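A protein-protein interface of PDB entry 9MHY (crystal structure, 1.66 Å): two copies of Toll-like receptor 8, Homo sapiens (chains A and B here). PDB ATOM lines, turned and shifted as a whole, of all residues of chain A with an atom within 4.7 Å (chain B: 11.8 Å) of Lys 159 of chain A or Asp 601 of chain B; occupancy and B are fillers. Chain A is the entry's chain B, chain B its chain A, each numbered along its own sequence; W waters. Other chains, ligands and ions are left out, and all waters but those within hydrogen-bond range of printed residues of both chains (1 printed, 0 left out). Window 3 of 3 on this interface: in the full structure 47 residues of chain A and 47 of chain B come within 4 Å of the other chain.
OD2 of Asp 601 of chain B is in hydrogen-bond range of OH of Tyr 156 of chain A. N of Asn 158 of chain A lies within hydrogen-bond range of O of Asp 601 of chain B (2.9 Å). The side-chain amide oxygen (OD1) of Asn 158 of chain A sits at hydrogen-bond distance from the backbone NH (N) of Asn 603 of chain B (3.0 Å).
OD1 of Asn 599 of chain B lies within hydrogen-bond range of N of Asp 601 of chain B, at 2.9 Å. OD2 of Asp 602 of chain B is in salt-bridge range of NH2 of Arg 604 of chain B. The side-chain amino group (NZ) of Lys 159 of chain A is in hydrogen-bond range of the backbone carbonyl oxygen (O) of Asn 130 of chain A, at 2.8 Å. OD1 of Asn 131 of chain A lies within hydrogen-bond range of NZ of Lys 159 of chain A, 2.8 Å away. The side-chain amino group (NZ) of Lys 159 of chain A is in hydrogen-bond range of the backbone carbonyl oxygen (O) of Asn 154 of chain A. SG of Cys 155 of chain A is disulfide-bonded to SG of Cys 161 of chain A, at 2.0 Å.
Among the printed residues, merely in contact across the chains: Pro 240 of chain A with Asp 602 of chain B (3.3 Å), Phe 157 of chain A with Asp 601 of chain B (3.3 Å), Pro 240 of chain A with Asp 601 of chain B (3.6 Å), Lys 159 of chain A with Asp 601 of chain B (3.7 Å), Asn 158 of chain A with Asp 602 of chain B (3.7 Å) and Pro 240 of chain A with Arg 604 of chain B (3.8 Å).
Asn 131 of chain A touches none of the printed residues of chain B. No residue of chain B comes within 4 Å of Cys 155 of chain A. Of chain B, only Asp 601 (2.8 Å) comes within 4 Å of Tyr 156 of chain A. Asn 158 of chain A touches three residues of chain B. Pro 240 of chain A touches just these residues of chain B: Asp 601 (3.6 Å), Asp 602 (3.3 Å) and Arg 604 (3.8 Å). Asp 601 of chain B touches just these residues of chain A: Tyr 156, Phe 157, Asn 158, Lys 159 and Pro 240. Of the printed residues of chain A, Asp 602 of chain B touches Asn 158 (3.7 Å) and Pro 240 (3.3 Å). Of the printed residues of chain A, Asn 603 of chain B touches Asn 158 (3.0 Å). Of the printed residues of chain A, Arg 604 of chain B touches Pro 240. The nearest printed residue of chain A that does not touch Arg 604 of chain B is Asn 158 of chain A (4.6 Å).
Of the 12 printed residues of chain A, 5 touch a printed residue of chain B. Hydrophobic or aromatic side chains of chain A that line the printed part of chain B: Tyr 156, Phe 157 and Pro 240. Of the 22 printed residues of chain B, 4 touch a printed residue of chain A. Printed residues of chain B that touch a printed residue of chain A: Asp 601, Asp 602, Asn 603 and Arg 604. Along chain B the printed residues that touch a printed residue of chain A span positions 601 to 604. Among the printed residues, 9 pairs touch across the chains. Among the printed residues, no Asp or Glu carboxylate lies within 4 Å of a Lys or Arg side-chain nitrogen of the other chain.
No position is printed for both chains. Of the 9 pairs that touch across the chains among the printed residues, none has its exchanged pair printed and touching as well.
Water W1 bridges the side-chain amide nitrogen of Asn 603 of chain B (2.8 Å) and the backbone carbonyl oxygen of Asn 158 of chain A (3.1 Å).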
ATOM      1  N   ASN A 130     -24.390 -16.945 -23.437  1.00  0.00           N
ATOM      2  CA  ASN A 130     -23.598 -16.655 -24.630  1.00  0.00           C
ATOM      3  C   ASN A 130     -22.210 -16.115 -24.168  1.00  0.00           C
ATOM      4  O   ASN A 130     -21.853 -16.311 -23.002  1.00  0.00           O
ATOM      5  CB  ASN A 130     -24.378 -15.687 -25.534  1.00  0.00           C
ATOM      6  CG  ASN A 130     -25.470 -16.387 -26.286  1.00  0.00           C
ATOM      7  OD1 ASN A 130     -25.208 -17.223 -27.137  1.00  0.00           O
ATOM      8  ND2 ASN A 130     -26.702 -16.060 -26.005  1.00  0.00           N
ATOM      9  N   ASN A 131     -21.405 -15.521 -25.076  1.00  0.00           N
ATOM     10  CA  ASN A 131     -20.098 -14.944 -24.753  1.00  0.00           C
ATOM     11  C   ASN A 131     -20.144 -13.428 -24.984  1.00  0.00           C
ATOM     12  O   ASN A 131     -19.182 -12.856 -25.493  1.00  0.00           O
ATOM     13  CB  ASN A 131     -19.029 -15.594 -25.637  1.00  0.00           C
ATOM     14  CG  ASN A 131     -18.976 -17.101 -25.488  1.00  0.00           C
ATOM     15  OD1 ASN A 131     -19.264 -17.656 -24.421  1.00  0.00           O
ATOM     16  ND2 ASN A 131     -18.601 -17.801 -26.550  1.00  0.00           N
ATOM     17  N   TYR A 133     -19.872  -9.809 -23.786  1.00  0.00           N
ATOM     18  CA  TYR A 133     -19.253  -9.027 -22.707  1.00  0.00           C
ATOM     19  C   TYR A 133     -19.372  -7.512 -22.948  1.00  0.00           C
ATOM     20  O   TYR A 133     -18.777  -6.754 -22.203  1.00  0.00           O
ATOM     21  CB  TYR A 133     -17.760  -9.420 -22.550  1.00  0.00           C
ATOM     22  CG  TYR A 133     -17.528 -10.918 -22.587  1.00  0.00           C
ATOM     23  CD1 TYR A 133     -18.304 -11.778 -21.827  1.00  0.00           C
ATOM     24  CD2 TYR A 133     -16.584 -11.477 -23.439  1.00  0.00           C
ATOM     25  CE1 TYR A 133     -18.202 -13.155 -21.964  1.00  0.00           C
ATOM     26  CE2 TYR A 133     -16.408 -12.857 -23.516  1.00  0.00           C
ATOM     27  CZ  TYR A 133     -17.237 -13.695 -22.792  1.00  0.00           C
ATOM     28  OH  TYR A 133     -17.112 -15.068 -22.840  1.00  0.00           O
ATOM     29  N   ASN A 154     -23.424 -14.867 -18.966  1.00  0.00           N
ATOM     30  CA  ASN A 154     -22.455 -14.710 -20.054  1.00  0.00           C
ATOM     31  C   ASN A 154     -21.020 -14.745 -19.496  1.00  0.00           C
ATOM     32  O   ASN A 154     -20.123 -15.131 -20.230  1.00  0.00           O
ATOM     33  CB  ASN A 154     -22.725 -13.449 -20.914  1.00  0.00           C
ATOM     34  CG  ASN A 154     -23.826 -13.649 -21.932  1.00  0.00           C
ATOM     35  OD1 ASN A 154     -23.584 -13.685 -23.133  1.00  0.00           O
ATOM     36  ND2 ASN A 154     -25.047 -13.853 -21.481  1.00  0.00           N
ATOM     37  N   CYS A 155     -20.796 -14.388 -18.214  1.00  0.00           N
ATOM     38  CA  CYS A 155     -19.454 -14.430 -17.633  1.00  0.00           C
ATOM     39  C   CYS A 155     -19.554 -14.750 -16.139  1.00  0.00           C
ATOM     40  O   CYS A 155     -19.994 -13.915 -15.359  1.00  0.00           O
ATOM     41  CB  CYS A 155     -18.720 -13.115 -17.875  1.00  0.00           C
ATOM     42  SG  CYS A 155     -17.027 -13.098 -17.241  1.00  0.00           S
ATOM     43  N   TYR A 156     -19.156 -15.956 -15.736  1.00  0.00           N
ATOM     44  CA  TYR A 156     -19.355 -16.404 -14.360  1.00  0.00           C
ATOM     45  C   TYR A 156     -18.455 -17.573 -13.996  1.00  0.00           C
ATOM     46  O   TYR A 156     -17.887 -18.204 -14.886  1.00  0.00           O
ATOM     47  CB  TYR A 156     -20.836 -16.838 -14.204  1.00  0.00           C
ATOM     48  CG  TYR A 156     -21.195 -17.948 -15.164  1.00  0.00           C
ATOM     49  CD1 TYR A 156     -21.530 -17.671 -16.484  1.00  0.00           C
ATOM     50  CD2 TYR A 156     -21.038 -19.278 -14.803  1.00  0.00           C
ATOM     51  CE1 TYR A 156     -21.742 -18.690 -17.403  1.00  0.00           C
ATOM     52  CE2 TYR A 156     -21.277 -20.305 -15.703  1.00  0.00           C
ATOM     53  CZ  TYR A 156     -21.629 -20.008 -17.007  1.00  0.00           C
ATOM     54  OH  TYR A 156     -21.885 -21.017 -17.906  1.00  0.00           O
ATOM     55  N   PHE A 157     -18.322 -17.853 -12.678  1.00  0.00           N
ATOM     56  CA  PHE A 157     -17.544 -18.976 -12.138  1.00  0.00           C
ATOM     57  C   PHE A 157     -16.094 -18.938 -12.701  1.00  0.00           C
ATOM     58  O   PHE A 157     -15.506 -17.855 -12.670  1.00  0.00           O
ATOM     59  CB  PHE A 157     -18.307 -20.304 -12.406  1.00  0.00           C
ATOM     60  CG  PHE A 157     -19.667 -20.498 -11.779  1.00  0.00           C
ATOM     61  CD1 PHE A 157     -20.164 -19.595 -10.855  1.00  0.00           C
ATOM     62  CD2 PHE A 157     -20.473 -21.554 -12.158  1.00  0.00           C
ATOM     63  CE1 PHE A 157     -21.437 -19.760 -10.315  1.00  0.00           C
ATOM     64  CE2 PHE A 157     -21.737 -21.716 -11.607  1.00  0.00           C
ATOM     65  CZ  PHE A 157     -22.199 -20.827 -10.675  1.00  0.00           C
ATOM     66  N   ASN A 158     -15.532 -20.043 -13.242  1.00  0.00           N
ATOM     67  CA  ASN A 158     -14.191 -20.031 -13.817  1.00  0.00           C
ATOM     68  C   ASN A 158     -14.215 -19.983 -15.346  1.00  0.00           C
ATOM     69  O   ASN A 158     -13.193 -20.268 -15.968  1.00  0.00           O
ATOM     70  CB  ASN A 158     -13.384 -21.237 -13.333  1.00  0.00           C
ATOM     71  CG  ASN A 158     -13.203 -21.293 -11.835  1.00  0.00           C
ATOM     72  OD1 ASN A 158     -13.400 -22.335 -11.211  1.00  0.00           O
ATOM     73  ND2 ASN A 158     -12.752 -20.204 -11.215  1.00  0.00           N
ATOM     74  N   LYS A 159     -15.324 -19.527 -15.969  1.00  0.00           N
ATOM     75  CA  LYS A 159     -15.364 -19.352 -17.419  1.00  0.00           C
ATOM     76  C   LYS A 159     -14.318 -18.304 -17.827  1.00  0.00           C
ATOM     77  O   LYS A 159     -14.115 -17.317 -17.114  1.00  0.00           O
ATOM     78  CB  LYS A 159     -16.753 -18.865 -17.870  1.00  0.00           C
ATOM     79  CG  LYS A 159     -16.887 -18.704 -19.377  1.00  0.00           C
ATOM     80  CD  LYS A 159     -18.280 -18.212 -19.766  1.00  0.00           C
ATOM     81  CE  LYS A 159     -18.333 -17.896 -21.237  1.00  0.00           C
ATOM     82  NZ  LYS A 159     -19.681 -17.435 -21.664  1.00  0.00           N
ATOM     83  N   VAL A 160     -13.630 -18.543 -18.942  1.00  0.00           N
ATOM     84  CA  VAL A 160     -12.651 -17.593 -19.454  1.00  0.00           C
ATOM     85  C   VAL A 160     -13.504 -16.542 -20.136  1.00  0.00           C
ATOM     86  O   VAL A 160     -14.166 -16.852 -21.125  1.00  0.00           O
ATOM     87  CB  VAL A 160     -11.638 -18.232 -20.426  1.00  0.00           C
ATOM     88  CG1 VAL A 160     -10.650 -17.179 -20.939  1.00  0.00           C
ATOM     89  CG2 VAL A 160     -10.899 -19.397 -19.756  1.00  0.00           C
ATOM     90  N   CYS A 161     -13.601 -15.357 -19.539  1.00  0.00           N
ATOM     91  CA  CYS A 161     -14.471 -14.312 -20.062  1.00  0.00           C
ATOM     92  C   CYS A 161     -14.031 -12.941 -19.575  1.00  0.00           C
ATOM     93  O   CYS A 161     -13.345 -12.817 -18.562  1.00  0.00           O
ATOM     94  CB  CYS A 161     -15.926 -14.599 -19.690  1.00  0.00           C
ATOM     95  SG  CYS A 161     -16.219 -14.846 -17.919  1.00  0.00           S
ATOM     96  N   PRO A 240     -17.792 -22.689  -8.074  1.00  0.00           N
ATOM     97  CA  PRO A 240     -16.629 -21.831  -7.763  1.00  0.00           C
ATOM     98  C   PRO A 240     -17.111 -20.511  -7.167  1.00  0.00           C
ATOM     99  O   PRO A 240     -17.918 -19.818  -7.776  1.00  0.00           O
ATOM    100  CB  PRO A 240     -15.952 -21.640  -9.127  1.00  0.00           C
ATOM    101  CG  PRO A 240     -16.461 -22.748  -9.958  1.00  0.00           C
ATOM    102  CD  PRO A 240     -17.895 -22.914  -9.527  1.00  0.00           C
ATOM    103  N   TYR B 571     -20.837 -35.352  -6.237  1.00  0.00           N
ATOM    104  CA  TYR B 571     -20.753 -34.167  -7.092  1.00  0.00           C
ATOM    105  C   TYR B 571     -20.173 -32.950  -6.400  1.00  0.00           C
ATOM    106  O   TYR B 571     -20.002 -31.942  -7.064  1.00  0.00           O
ATOM    107  CB  TYR B 571     -22.122 -33.792  -7.678  1.00  0.00           C
ATOM    108  CG  TYR B 571     -23.117 -33.198  -6.706  1.00  0.00           C
ATOM    109  CD1 TYR B 571     -23.836 -34.013  -5.848  1.00  0.00           C
ATOM    110  CD2 TYR B 571     -23.496 -31.864  -6.800  1.00  0.00           C
ATOM    111  CE1 TYR B 571     -24.860 -33.514  -5.063  1.00  0.00           C
ATOM    112  CE2 TYR B 571     -24.530 -31.349  -6.018  1.00  0.00           C
ATOM    113  CZ  TYR B 571     -25.220 -32.187  -5.160  1.00  0.00           C
ATOM    114  OH  TYR B 571     -26.275 -31.739  -4.412  1.00  0.00           O
ATOM    115  N   TYR B 577     -10.629 -31.073  -2.597  1.00  0.00           N
ATOM    116  CA  TYR B 577     -11.306 -31.505  -3.820  1.00  0.00           C
ATOM    117  C   TYR B 577     -10.645 -32.721  -4.496  1.00  0.00           C
ATOM    118  O   TYR B 577     -11.233 -33.291  -5.426  1.00  0.00           O
ATOM    119  CB  TYR B 577     -11.333 -30.320  -4.795  1.00  0.00           C
ATOM    120  CG  TYR B 577     -11.951 -29.075  -4.196  1.00  0.00           C
ATOM    121  CD1 TYR B 577     -13.234 -29.097  -3.677  1.00  0.00           C
ATOM    122  CD2 TYR B 577     -11.237 -27.884  -4.118  1.00  0.00           C
ATOM    123  CE1 TYR B 577     -13.824 -27.953  -3.159  1.00  0.00           C
ATOM    124  CE2 TYR B 577     -11.814 -26.732  -3.595  1.00  0.00           C
ATOM    125  CZ  TYR B 577     -13.121 -26.764  -3.141  1.00  0.00           C
ATOM    126  OH  TYR B 577     -13.694 -25.647  -2.572  1.00  0.00           O
ATOM    127  N   LEU B 594     -19.184 -37.022 -12.418  1.00  0.00           N
ATOM    128  CA  LEU B 594     -18.063 -36.316 -13.034  1.00  0.00           C
ATOM    129  C   LEU B 594     -18.539 -35.290 -14.080  1.00  0.00           C
ATOM    130  O   LEU B 594     -17.793 -34.361 -14.385  1.00  0.00           O
ATOM    131  CB  LEU B 594     -17.019 -37.264 -13.631  1.00  0.00           C
ATOM    132  CG  LEU B 594     -16.140 -37.998 -12.622  1.00  0.00           C
ATOM    133  CD1 LEU B 594     -15.503 -39.202 -13.249  1.00  0.00           C
ATOM    134  CD2 LEU B 594     -15.052 -37.067 -12.060  1.00  0.00           C
ATOM    135  N   ASP B 595     -19.788 -35.401 -14.591  1.00  0.00           N
ATOM    136  CA  ASP B 595     -20.330 -34.354 -15.481  1.00  0.00           C
ATOM    137  C   ASP B 595     -20.419 -33.020 -14.710  1.00  0.00           C
ATOM    138  O   ASP B 595     -20.131 -31.964 -15.278  1.00  0.00           O
ATOM    139  CB  ASP B 595     -21.716 -34.737 -16.028  1.00  0.00           C
ATOM    140  CG  ASP B 595     -22.813 -34.877 -14.973  1.00  0.00           C
ATOM    141  OD1 ASP B 595     -22.565 -35.554 -13.933  1.00  0.00           O
ATOM    142  OD2 ASP B 595     -23.928 -34.353 -15.202  1.00  0.00           O
ATOM    143  N   ILE B 596     -20.763 -33.075 -13.404  1.00  0.00           N
ATOM    144  CA  ILE B 596     -20.821 -31.887 -12.555  1.00  0.00           C
ATOM    145  C   ILE B 596     -19.409 -31.513 -12.061  1.00  0.00           C
ATOM    146  O   ILE B 596     -19.019 -30.351 -12.170  1.00  0.00           O
ATOM    147  CB  ILE B 596     -21.810 -32.100 -11.374  1.00  0.00           C
ATOM    148  CG1 ILE B 596     -23.260 -32.197 -11.912  1.00  0.00           C
ATOM    149  CG2 ILE B 596     -21.653 -30.970 -10.326  1.00  0.00           C
ATOM    150  CD1 ILE B 596     -24.345 -32.522 -10.863  1.00  0.00           C
ATOM    151  N   LEU B 597     -18.651 -32.479 -11.499  1.00  0.00           N
ATOM    152  CA  LEU B 597     -17.296 -32.189 -10.999  1.00  0.00           C
ATOM    153  C   LEU B 597     -16.390 -31.577 -12.073  1.00  0.00           C
ATOM    154  O   LEU B 597     -15.625 -30.661 -11.785  1.00  0.00           O
ATOM    155  CB  LEU B 597     -16.633 -33.453 -10.415  1.00  0.00           C
ATOM    156  CG  LEU B 597     -17.359 -34.116  -9.229  1.00  0.00           C
ATOM    157  CD1 LEU B 597     -17.045 -35.625  -9.111  1.00  0.00           C
ATOM    158  CD2 LEU B 597     -16.995 -33.420  -7.936  1.00  0.00           C
ATOM    159  N   TRP B 598     -16.494 -32.075 -13.315  1.00  0.00           N
ATOM    160  CA  TRP B 598     -15.696 -31.578 -14.432  1.00  0.00           C
ATOM    161  C   TRP B 598     -16.492 -30.646 -15.345  1.00  0.00           C
ATOM    162  O   TRP B 598     -16.162 -30.503 -16.521  1.00  0.00           O
ATOM    163  CB  TRP B 598     -15.101 -32.742 -15.232  1.00  0.00           C
ATOM    164  CG  TRP B 598     -14.021 -33.499 -14.521  1.00  0.00           C
ATOM    165  CD1 TRP B 598     -13.142 -33.013 -13.593  1.00  0.00           C
ATOM    166  CD2 TRP B 598     -13.564 -34.815 -14.854  1.00  0.00           C
ATOM    167  NE1 TRP B 598     -12.242 -33.993 -13.242  1.00  0.00           N
ATOM    168  CE2 TRP B 598     -12.441 -35.087 -14.045  1.00  0.00           C
ATOM    169  CE3 TRP B 598     -13.981 -35.779 -15.777  1.00  0.00           C
ATOM    170  CZ2 TRP B 598     -11.801 -36.322 -14.062  1.00  0.00           C
ATOM    171  CZ3 TRP B 598     -13.341 -37.000 -15.794  1.00  0.00           C
ATOM    172  CH2 TRP B 598     -12.227 -37.241 -14.990  1.00  0.00           C
ATOM    173  N   ASN B 599     -17.467 -29.915 -14.790  1.00  0.00           N
ATOM    174  CA  ASN B 599     -18.214 -28.911 -15.553  1.00  0.00           C
ATOM    175  C   ASN B 599     -17.225 -27.866 -16.104  1.00  0.00           C
ATOM    176  O   ASN B 599     -16.277 -27.500 -15.398  1.00  0.00           O
ATOM    177  CB  ASN B 599     -19.240 -28.234 -14.647  1.00  0.00           C
ATOM    178  CG  ASN B 599     -19.974 -27.119 -15.320  1.00  0.00           C
ATOM    179  OD1 ASN B 599     -19.540 -25.955 -15.274  1.00  0.00           O
ATOM    180  ND2 ASN B 599     -21.078 -27.454 -15.981  1.00  0.00           N
ATOM    181  N   ASP B 600     -17.385 -27.471 -17.375  1.00  0.00           N
ATOM    182  CA  ASP B 600     -16.474 -26.535 -18.049  1.00  0.00           C
ATOM    183  C   ASP B 600     -16.198 -25.240 -17.284  1.00  0.00           C
ATOM    184  O   ASP B 600     -15.169 -24.614 -17.521  1.00  0.00           O
ATOM    185  CB  ASP B 600     -17.035 -26.137 -19.424  1.00  0.00           C
ATOM    186  CG  ASP B 600     -17.039 -27.229 -20.463  1.00  0.00           C
ATOM    187  OD1 ASP B 600     -16.247 -28.186 -20.323  1.00  0.00           O
ATOM    188  OD2 ASP B 600     -17.837 -27.133 -21.420  1.00  0.00           O
ATOM    189  N   ASP B 601     -17.135 -24.800 -16.440  1.00  0.00           N
ATOM    190  CA  ASP B 601     -16.999 -23.536 -15.712  1.00  0.00           C
ATOM    191  C   ASP B 601     -16.419 -23.710 -14.295  1.00  0.00           C
ATOM    192  O   ASP B 601     -16.406 -22.744 -13.543  1.00  0.00           O
ATOM    193  CB  ASP B 601     -18.375 -22.852 -15.628  1.00  0.00           C
ATOM    194  CG  ASP B 601     -19.057 -22.700 -16.972  1.00  0.00           C
ATOM    195  OD1 ASP B 601     -18.445 -22.115 -17.881  1.00  0.00           O
ATOM    196  OD2 ASP B 601     -20.222 -23.170 -17.111  1.00  0.00           O
ATOM    197  N   ASP B 602     -15.919 -24.909 -13.937  1.00  0.00           N
ATOM    198  CA  ASP B 602     -15.353 -25.157 -12.617  1.00  0.00           C
ATOM    199  C   ASP B 602     -13.970 -25.789 -12.747  1.00  0.00           C
ATOM    200  O   ASP B 602     -13.841 -26.862 -13.332  1.00  0.00           O
ATOM    201  CB  ASP B 602     -16.296 -26.091 -11.828  1.00  0.00           C
ATOM    202  CG  ASP B 602     -15.957 -26.273 -10.362  1.00  0.00           C
ATOM    203  OD1 ASP B 602     -14.981 -25.663  -9.897  1.00  0.00           O
ATOM    204  OD2 ASP B 602     -16.686 -27.013  -9.673  1.00  0.00           O
ATOM    205  N   ASN B 603     -12.943 -25.146 -12.175  1.00  0.00           N
ATOM    206  CA  ASN B 603     -11.583 -25.693 -12.189  1.00  0.00           C
ATOM    207  C   ASN B 603     -11.234 -26.459 -10.902  1.00  0.00           C
ATOM    208  O   ASN B 603     -10.117 -26.980 -10.818  1.00  0.00           O
ATOM    209  CB  ASN B 603     -10.569 -24.547 -12.371  1.00  0.00           C
ATOM    210  CG  ASN B 603     -10.637 -23.892 -13.732  1.00  0.00           C
ATOM    211  OD1 ASN B 603     -11.071 -24.503 -14.721  1.00  0.00           O
ATOM    212  ND2 ASN B 603     -10.177 -22.640 -13.825  1.00  0.00           N
ATOM    213  N   ARG B 604     -12.135 -26.521  -9.897  1.00  0.00           N
ATOM    214  CA  ARG B 604     -11.770 -27.090  -8.595  1.00  0.00           C
ATOM    215  C   ARG B 604     -11.415 -28.591  -8.581  1.00  0.00           C
ATOM    216  O   ARG B 604     -10.563 -28.973  -7.782  1.00  0.00           O
ATOM    217  CB  ARG B 604     -12.851 -26.814  -7.544  1.00  0.00           C
ATOM    218  CG  ARG B 604     -13.018 -25.311  -7.225  1.00  0.00           C
ATOM    219  CD  ARG B 604     -14.236 -25.024  -6.347  1.00  0.00           C
ATOM    220  NE  ARG B 604     -15.452 -25.516  -6.988  1.00  0.00           N
ATOM    221  CZ  ARG B 604     -16.562 -25.895  -6.361  1.00  0.00           C
ATOM    222  NH1 ARG B 604     -16.650 -25.812  -5.035  1.00  0.00           N
ATOM    223  NH2 ARG B 604     -17.582 -26.392  -7.052  1.00  0.00           N
ATOM    224  N   TYR B 605     -12.027 -29.403  -9.438  1.00  0.00           N
ATOM    225  CA  TYR B 605     -11.815 -30.868  -9.469  1.00  0.00           C
ATOM    226  C   TYR B 605     -11.003 -31.339 -10.673  1.00  0.00           C
ATOM    227  O   TYR B 605     -10.970 -32.535 -10.944  1.00  0.00           O
ATOM    228  CB  TYR B 605     -13.177 -31.584  -9.477  1.00  0.00           C
ATOM    229  CG  TYR B 605     -14.028 -31.208  -8.291  1.00  0.00           C
ATOM    230  CD1 TYR B 605     -13.891 -31.868  -7.076  1.00  0.00           C
ATOM    231  CD2 TYR B 605     -14.919 -30.144  -8.359  1.00  0.00           C
ATOM    232  CE1 TYR B 605     -14.674 -31.529  -5.978  1.00  0.00           C
ATOM    233  CE2 TYR B 605     -15.695 -29.784  -7.263  1.00  0.00           C
ATOM    234  CZ  TYR B 605     -15.562 -30.472  -6.071  1.00  0.00           C
ATOM    235  OH  TYR B 605     -16.309 -30.115  -4.972  1.00  0.00           O
ATOM    236  N   ILE B 606     -10.272 -30.420 -11.325  1.00  0.00           N
ATOM    237  CA  ILE B 606      -9.513 -30.715 -12.529  1.00  0.00           C
ATOM    238  C   ILE B 606      -8.356 -31.716 -12.280  1.00  0.00           C
ATOM    239  O   ILE B 606      -7.909 -32.346 -13.230  1.00  0.00           O
ATOM    240  CB  ILE B 606      -9.026 -29.377 -13.206  1.00  0.00           C
ATOM    241  CG1 ILE B 606      -8.895 -29.540 -14.728  1.00  0.00           C
ATOM    242  CG2 ILE B 606      -7.722 -28.870 -12.595  1.00  0.00           C
ATOM    243  CD1 ILE B 606     -10.269 -29.422 -15.502  1.00  0.00           C
ATOM    244  N   LEU B 625     -21.123 -38.271 -18.453  1.00  0.00           N
ATOM    245  CA  LEU B 625     -20.175 -37.407 -19.139  1.00  0.00           C
ATOM    246  C   LEU B 625     -20.508 -37.195 -20.609  1.00  0.00           C
ATOM    247  O   LEU B 625     -20.682 -38.157 -21.342  1.00  0.00           O
ATOM    248  CB  LEU B 625     -18.740 -37.990 -19.011  1.00  0.00           C
ATOM    249  CG  LEU B 625     -18.087 -37.859 -17.622  1.00  0.00           C
ATOM    250  CD1 LEU B 625     -16.944 -38.841 -17.459  1.00  0.00           C
ATOM    251  CD2 LEU B 625     -17.560 -36.446 -17.405  1.00  0.00           C
ATOM    252  N   HIS B 627     -18.488 -34.753 -22.322  1.00  0.00           N
ATOM    253  CA  HIS B 627     -17.109 -34.528 -22.749  1.00  0.00           C
ATOM    254  C   HIS B 627     -16.226 -34.389 -21.498  1.00  0.00           C
ATOM    255  O   HIS B 627     -16.725 -34.041 -20.424  1.00  0.00           O
ATOM    256  CB  HIS B 627     -17.014 -33.271 -23.622  1.00  0.00           C
ATOM    257  CG  HIS B 627     -17.372 -32.030 -22.880  1.00  0.00           C
ATOM    258  ND1 HIS B 627     -18.688 -31.681 -22.651  1.00  0.00           N
ATOM    259  CD2 HIS B 627     -16.567 -31.114 -22.296  1.00  0.00           C
ATOM    260  CE1 HIS B 627     -18.650 -30.560 -21.953  1.00  0.00           C
ATOM    261  NE2 HIS B 627     -17.391 -30.184 -21.709  1.00  0.00           N
ATOM    262  N   ILE B 628     -14.941 -34.693 -21.622  1.00  0.00           N
ATOM    263  CA  ILE B 628     -14.007 -34.557 -20.509  1.00  0.00           C
ATOM    264  C   ILE B 628     -13.142 -33.353 -20.855  1.00  0.00           C
ATOM    265  O   ILE B 628     -12.550 -33.356 -21.940  1.00  0.00           O
ATOM    266  CB  ILE B 628     -13.143 -35.827 -20.321  1.00  0.00           C
ATOM    267  CG1 ILE B 628     -14.045 -37.032 -19.922  1.00  0.00           C
ATOM    268  CG2 ILE B 628     -12.055 -35.564 -19.258  1.00  0.00           C
ATOM    269  CD1 ILE B 628     -13.454 -38.373 -20.182  1.00  0.00           C
ATOM    270  N   PRO B 629     -12.999 -32.323 -19.983  1.00  0.00           N
ATOM    271  CA  PRO B 629     -12.108 -31.197 -20.339  1.00  0.00           C
ATOM    272  C   PRO B 629     -10.693 -31.702 -20.603  1.00  0.00           C
ATOM    273  O   PRO B 629     -10.230 -32.611 -19.909  1.00  0.00           O
ATOM    274  CB  PRO B 629     -12.152 -30.294 -19.105  1.00  0.00           C
ATOM    275  CG  PRO B 629     -13.376 -30.679 -18.375  1.00  0.00           C
ATOM    276  CD  PRO B 629     -13.601 -32.127 -18.649  1.00  0.00           C
ATOM    277  N   ASN B 630     -10.022 -31.173 -21.622  1.00  0.00           N
ATOM    278  CA  ASN B 630      -8.671 -31.629 -21.981  1.00  0.00           C
ATOM    279  C   ASN B 630      -7.698 -31.625 -20.791  1.00  0.00           C
ATOM    280  O   ASN B 630      -6.984 -32.605 -20.583  1.00  0.00           O
ATOM    281  CB  ASN B 630      -8.131 -30.790 -23.133  1.00  0.00           C
ATOM    282  CG  ASN B 630      -8.969 -30.925 -24.392  1.00  0.00           C
ATOM    283  OD1 ASN B 630      -9.384 -32.025 -24.778  1.00  0.00           O
ATOM    284  ND2 ASN B 630      -9.249 -29.819 -25.064  1.00  0.00           N
ATOM    285  N   GLU B 631      -7.748 -30.576 -19.959  1.00  0.00           N
ATOM    286  CA  GLU B 631      -6.880 -30.466 -18.778  1.00  0.00           C
ATOM    287  C   GLU B 631      -7.213 -31.552 -17.749  1.00  0.00           C
ATOM    288  O   GLU B 631      -6.297 -32.069 -17.115  1.00  0.00           O
ATOM    289  CB  GLU B 631      -7.035 -29.074 -18.148  1.00  0.00           C
ATOM    290  CG  GLU B 631      -6.035 -28.734 -17.056  1.00  0.00           C
ATOM    291  CD  GLU B 631      -6.153 -27.315 -16.519  1.00  0.00           C
ATOM    292  OE1 GLU B 631      -7.160 -26.636 -16.829  1.00  0.00           O
ATOM    293  OE2 GLU B 631      -5.233 -26.881 -15.785  1.00  0.00           O
ATOM    294  N   ALA B 632      -8.512 -31.895 -17.579  1.00  0.00           N
ATOM    295  CA  ALA B 632      -8.898 -32.945 -16.638  1.00  0.00           C
ATOM    296  C   ALA B 632      -8.410 -34.305 -17.123  1.00  0.00           C
ATOM    297  O   ALA B 632      -7.951 -35.085 -16.295  1.00  0.00           O
ATOM    298  CB  ALA B 632     -10.407 -32.983 -16.440  1.00  0.00           C
HETATM  299  O   HOH W   1     -10.086 -20.643 -15.825  1.00  0.00           O
